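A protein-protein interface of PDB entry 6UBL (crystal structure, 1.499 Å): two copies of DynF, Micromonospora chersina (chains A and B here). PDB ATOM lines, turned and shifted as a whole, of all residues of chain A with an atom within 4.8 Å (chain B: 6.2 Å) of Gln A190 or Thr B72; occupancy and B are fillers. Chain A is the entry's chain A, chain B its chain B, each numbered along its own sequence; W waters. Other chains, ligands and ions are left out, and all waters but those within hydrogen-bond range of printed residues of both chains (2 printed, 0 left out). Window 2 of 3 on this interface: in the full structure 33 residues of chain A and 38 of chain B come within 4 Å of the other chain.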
ATOM      1  N   LEU A 182      22.006   3.842   1.468  1.00  0.00           N
ATOM      2  CA  LEU A 182      22.464   2.939   0.422  1.00  0.00           C
ATOM      3  C   LEU A 182      23.736   3.463  -0.231  1.00  0.00           C
ATOM      4  O   LEU A 182      23.910   4.673  -0.396  1.00  0.00           O
ATOM      5  CB  LEU A 182      21.382   2.832  -0.663  1.00  0.00           C
ATOM      6  CG  LEU A 182      19.972   2.519  -0.152  1.00  0.00           C
ATOM      7  CD1 LEU A 182      18.942   2.598  -1.264  1.00  0.00           C
ATOM      8  CD2 LEU A 182      19.987   1.149   0.497  1.00  0.00           C
ATOM      9  N   ASP A 188      20.648  -0.791  -5.359  1.00  0.00           N
ATOM     10  CA  ASP A 188      19.732  -1.914  -5.215  1.00  0.00           C
ATOM     11  C   ASP A 188      20.247  -2.946  -4.216  1.00  0.00           C
ATOM     12  O   ASP A 188      19.643  -4.020  -4.085  1.00  0.00           O
ATOM     13  CB  ASP A 188      19.538  -2.666  -6.540  1.00  0.00           C
ATOM     14  CG  ASP A 188      18.664  -1.931  -7.547  1.00  0.00           C
ATOM     15  OD1 ASP A 188      17.902  -1.017  -7.193  1.00  0.00           O
ATOM     16  OD2 ASP A 188      18.717  -2.321  -8.736  1.00  0.00           O
ATOM     17  N   GLY A 189      21.367  -2.664  -3.537  1.00  0.00           N
ATOM     18  CA  GLY A 189      21.942  -3.603  -2.601  1.00  0.00           C
ATOM     19  C   GLY A 189      21.380  -3.444  -1.203  1.00  0.00           C
ATOM     20  O   GLY A 189      20.472  -2.655  -0.948  1.00  0.00           O
ATOM     21  N   GLN A 190      21.928  -4.230  -0.279  1.00  0.00           N
ATOM     22  CA  GLN A 190      21.558  -4.050   1.117  1.00  0.00           C
ATOM     23  C   GLN A 190      22.022  -2.674   1.586  1.00  0.00           C
ATOM     24  O   GLN A 190      23.056  -2.170   1.134  1.00  0.00           O
ATOM     25  CB  GLN A 190      22.217  -5.110   2.003  1.00  0.00           C
ATOM     26  CG  GLN A 190      21.662  -6.513   1.848  1.00  0.00           C
ATOM     27  CD  GLN A 190      21.865  -7.376   3.085  1.00  0.00           C
ATOM     28  OE1 GLN A 190      21.924  -6.875   4.211  1.00  0.00           O
ATOM     29  NE2 GLN A 190      21.961  -8.683   2.877  1.00  0.00           N
ATOM     30  N   PRO A 191      21.293  -2.050   2.507  1.00  0.00           N
ATOM     31  CA  PRO A 191      21.788  -0.805   3.104  1.00  0.00           C
ATOM     32  C   PRO A 191      23.155  -1.002   3.742  1.00  0.00           C
ATOM     33  O   PRO A 191      23.471  -2.071   4.264  1.00  0.00           O
ATOM     34  CB  PRO A 191      20.712  -0.451   4.146  1.00  0.00           C
ATOM     35  CG  PRO A 191      19.452  -1.094   3.592  1.00  0.00           C
ATOM     36  CD  PRO A 191      19.937  -2.389   2.981  1.00  0.00           C
ATOM     37  N   VAL A 192      23.989   0.031   3.631  1.00  0.00           N
ATOM     38  CA  VAL A 192      25.297   0.042   4.282  1.00  0.00           C
ATOM     39  C   VAL A 192      25.193   0.505   5.725  1.00  0.00           C
ATOM     40  O   VAL A 192      25.970   0.066   6.576  1.00  0.00           O
ATOM     41  CB  VAL A 192      26.239   0.969   3.489  1.00  0.00           C
ATOM     42  CG1 VAL A 192      27.559   1.159   4.232  1.00  0.00           C
ATOM     43  CG2 VAL A 192      26.455   0.440   2.090  1.00  0.00           C
ATOM     44  N   ARG B  11      14.533  -1.531  -1.731  1.00  0.00           N
ATOM     45  CA  ARG B  11      15.320  -2.507  -2.477  1.00  0.00           C
ATOM     46  C   ARG B  11      14.408  -3.412  -3.306  1.00  0.00           C
ATOM     47  O   ARG B  11      13.472  -4.020  -2.752  1.00  0.00           O
ATOM     48  CB  ARG B  11      16.076  -3.393  -1.501  1.00  0.00           C
ATOM     49  CG  ARG B  11      17.073  -4.272  -2.172  1.00  0.00           C
ATOM     50  CD  ARG B  11      17.809  -5.110  -1.178  1.00  0.00           C
ATOM     51  NE  ARG B  11      18.903  -5.801  -1.828  1.00  0.00           N
ATOM     52  CZ  ARG B  11      19.533  -6.860  -1.336  1.00  0.00           C
ATOM     53  NH1 ARG B  11      19.154  -7.365  -0.169  1.00  0.00           N
ATOM     54  NH2 ARG B  11      20.529  -7.420  -2.006  1.00  0.00           N
ATOM     55  N   SER B  69      12.376 -11.866  -0.126  1.00  0.00           N
ATOM     56  CA  SER B  69      13.651 -12.369  -0.609  1.00  0.00           C
ATOM     57  C   SER B  69      13.981 -13.652   0.150  1.00  0.00           C
ATOM     58  O   SER B  69      13.351 -13.956   1.167  1.00  0.00           O
ATOM     59  CB  SER B  69      14.748 -11.343  -0.326  1.00  0.00           C
ATOM     60  OG  SER B  69      15.014 -11.237   1.066  1.00  0.00           O
ATOM     61  N   PRO B  70      14.983 -14.414  -0.291  1.00  0.00           N
ATOM     62  CA  PRO B  70      15.497 -15.475   0.578  1.00  0.00           C
ATOM     63  C   PRO B  70      15.998 -14.831   1.859  1.00  0.00           C
ATOM     64  O   PRO B  70      16.414 -13.671   1.876  1.00  0.00           O
ATOM     65  CB  PRO B  70      16.650 -16.081  -0.230  1.00  0.00           C
ATOM     66  CG  PRO B  70      16.365 -15.702  -1.652  1.00  0.00           C
ATOM     67  CD  PRO B  70      15.734 -14.330  -1.558  1.00  0.00           C
ATOM     68  N   SER B  71      15.919 -15.571   2.952  1.00  0.00           N
ATOM     69  CA  SER B  71      16.481 -15.069   4.192  1.00  0.00           C
ATOM     70  C   SER B  71      17.999 -15.076   4.088  1.00  0.00           C
ATOM     71  O   SER B  71      18.590 -15.968   3.475  1.00  0.00           O
ATOM     72  CB  SER B  71      16.039 -15.920   5.370  1.00  0.00           C
ATOM     73  OG  SER B  71      16.661 -15.435   6.547  1.00  0.00           O
ATOM     74  N   THR B  72      18.636 -14.060   4.672  1.00  0.00           N
ATOM     75  CA  THR B  72      20.093 -14.036   4.693  1.00  0.00           C
ATOM     76  C   THR B  72      20.660 -15.121   5.597  1.00  0.00           C
ATOM     77  O   THR B  72      21.860 -15.403   5.526  1.00  0.00           O
ATOM     78  CB  THR B  72      20.602 -12.662   5.130  1.00  0.00           C
ATOM     79  OG1 THR B  72      20.144 -12.374   6.461  1.00  0.00           O
ATOM     80  CG2 THR B  72      20.110 -11.584   4.175  1.00  0.00           C
ATOM     81  N   SER B  73      19.827 -15.745   6.427  1.00  0.00           N
ATOM     82  CA  SER B  73      20.279 -16.842   7.266  1.00  0.00           C
ATOM     83  C   SER B  73      19.126 -17.782   7.581  1.00  0.00           C
ATOM     84  O   SER B  73      17.965 -17.370   7.646  1.00  0.00           O
ATOM     85  CB  SER B  73      20.861 -16.334   8.587  1.00  0.00           C
ATOM     86  OG  SER B  73      21.278 -17.418   9.400  1.00  0.00           O
ATOM     87  N   GLY B  74      19.465 -19.053   7.801  1.00  0.00           N
ATOM     88  CA  GLY B  74      18.501 -20.009   8.307  1.00  0.00           C
ATOM     89  C   GLY B  74      18.288 -19.965   9.805  1.00  0.00           C
ATOM     90  O   GLY B  74      17.340 -20.577  10.304  1.00  0.00           O
ATOM     91  N   ASP B  78      20.140 -14.148  13.031  1.00  0.00           N
ATOM     92  CA  ASP B  78      20.941 -13.524  11.988  1.00  0.00           C
ATOM     93  C   ASP B  78      20.119 -13.172  10.763  1.00  0.00           C
ATOM     94  O   ASP B  78      20.587 -12.406   9.918  1.00  0.00           O
ATOM     95  CB  ASP B  78      22.046 -14.496  11.549  1.00  0.00           C
ATOM     96  CG  ASP B  78      23.056 -14.764  12.649  1.00  0.00           C
ATOM     97  OD1 ASP B  78      23.299 -13.854  13.465  1.00  0.00           O
ATOM     98  OD2 ASP B  78      23.593 -15.890  12.708  1.00  0.00           O
ATOM     99  N   ALA B  79      18.892 -13.672  10.681  1.00  0.00           N
ATOM    100  CA  ALA B  79      18.130 -13.600   9.447  1.00  0.00           C
ATOM    101  C   ALA B  79      17.596 -12.197   9.209  1.00  0.00           C
ATOM    102  O   ALA B  79      17.050 -11.555  10.117  1.00  0.00           O
ATOM    103  CB  ALA B  79      16.975 -14.592   9.486  1.00  0.00           C
ATOM    104  N   GLU B  80      17.754 -11.731   7.975  1.00  0.00           N
ATOM    105  CA  GLU B  80      17.075 -10.553   7.479  1.00  0.00           C
ATOM    106  C   GLU B  80      16.305 -10.947   6.228  1.00  0.00           C
ATOM    107  O   GLU B  80      16.733 -11.821   5.462  1.00  0.00           O
ATOM    108  CB  GLU B  80      18.049  -9.476   7.034  1.00  0.00           C
ATOM    109  CG  GLU B  80      18.845  -8.823   8.113  1.00  0.00           C
ATOM    110  CD  GLU B  80      19.709  -7.739   7.516  1.00  0.00           C
ATOM    111  OE1 GLU B  80      19.161  -6.694   7.111  1.00  0.00           O
ATOM    112  OE2 GLU B  80      20.923  -7.967   7.402  1.00  0.00           O
ATOM    113  N   VAL B  81      15.166 -10.298   6.016  1.00  0.00           N
ATOM    114  CA  VAL B  81      14.337 -10.539   4.842  1.00  0.00           C
ATOM    115  C   VAL B  81      13.985  -9.188   4.233  1.00  0.00           C
ATOM    116  O   VAL B  81      13.652  -8.243   4.956  1.00  0.00           O
ATOM    117  CB  VAL B  81      13.069 -11.345   5.192  1.00  0.00           C
ATOM    118  CG1 VAL B  81      12.159 -11.441   3.977  1.00  0.00           C
ATOM    119  CG2 VAL B  81      13.449 -12.732   5.710  1.00  0.00           C
ATOM    120  N   TYR B  82      14.127  -9.081   2.916  1.00  0.00           N
ATOM    121  CA  TYR B  82      13.725  -7.906   2.155  1.00  0.00           C
ATOM    122  C   TYR B  82      12.403  -8.190   1.462  1.00  0.00           C
ATOM    123  O   TYR B  82      12.160  -9.308   1.002  1.00  0.00           O
ATOM    124  CB  TYR B  82      14.820  -7.540   1.157  1.00  0.00           C
ATOM    125  CG  TYR B  82      16.040  -7.027   1.884  1.00  0.00           C
ATOM    126  CD1 TYR B  82      16.999  -7.899   2.376  1.00  0.00           C
ATOM    127  CD2 TYR B  82      16.197  -5.672   2.125  1.00  0.00           C
ATOM    128  CE1 TYR B  82      18.107  -7.427   3.070  1.00  0.00           C
ATOM    129  CE2 TYR B  82      17.297  -5.190   2.809  1.00  0.00           C
ATOM    130  CZ  TYR B  82      18.244  -6.068   3.278  1.00  0.00           C
ATOM    131  OH  TYR B  82      19.334  -5.573   3.963  1.00  0.00           O
HETATM  132  O   HOH W   1      20.208  -9.778   1.040  1.00  0.00           O
HETATM  133  O   HOH W   2      20.978  -6.758  -4.818  1.00  0.00           O
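No position is printed for both chains.
NE of Arg B11 touches C of Gly A189, 3.5 Å away. CG of Gln A190 touches NH1 of Arg B11, at 3.3 Å. Gln A190 touches Thr B72. Glu B80 touches Gln A190. CD of Pro A191 touches OH of Tyr B82, at 3.4 Å.
The backbone NH of Glu B80 sits at hydrogen-bond distance from the side-chain hydroxyl of Thr B72, at 2.9 Å. The backbone NH (N) of Ser B69 sits at hydrogen-bond distance from the backbone carbonyl oxygen (O) of Tyr B82, at 2.8 Å. The backbone carbonyl oxygen (O) of Asp B78 sits at hydrogen-bond distance from the side-chain hydroxyl (OG1) of Thr B72 (3.5 Å). OE1 of Glu B80 lies within hydrogen-bond range of OH of Tyr B82.
Hydrophobic or aromatic side chains of chain A that line the printed part of chain B: Pro A191. Of the 12 printed residues of chain B, 4 touch a printed residue of chain A. Hydrophobic or aromatic side chains of chain B within 4 Å of the printed part of chain A: Tyr B82. Among the printed residues, no Asp or Glu carboxylate lies within 4 Å of a Lys or Arg side-chain nitrogen of the other chain.
Water W1 lies within hydrogen-bond range of NE2 of Gln A190 (2.8 Å) and NH1 of Arg B11 (2.9 Å). Water W2 bridges the guanidinium group of Arg B11 (2.9 Å) and the backbone carbonyl oxygen of Asp A188 (3.1 Å).
Of the printed residues of chain B, Asp A188 touches Arg B11. Of the printed residues of chain B, Gly A189 touches Arg B11 (3.5 Å). Gln A190 touches just these residues of chain B: Arg B11 (3.3 Å), Thr B72 (3.7 Å), Glu B80 (3.5 Å) and Tyr B82 (2.9 Å). Of chain A, only Gln A190 comes within 4 Å of Thr B72. Ala B79 touches none of the printed residues of chain A. The nearest printed residue of chain A that does not touch Glu B80 is Pro A191 (6.0 Å).
The side-chain amide oxygen (OE1) of Gln A190 is in hydrogen-bond range of the side-chain hydroxyl (OH) of Tyr B82 (2.9 Å). The guanidinium group of Arg B11 sits at hydrogen-bond distance from the backbone carbonyl oxygen of Asp A188 (3.0 Å).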
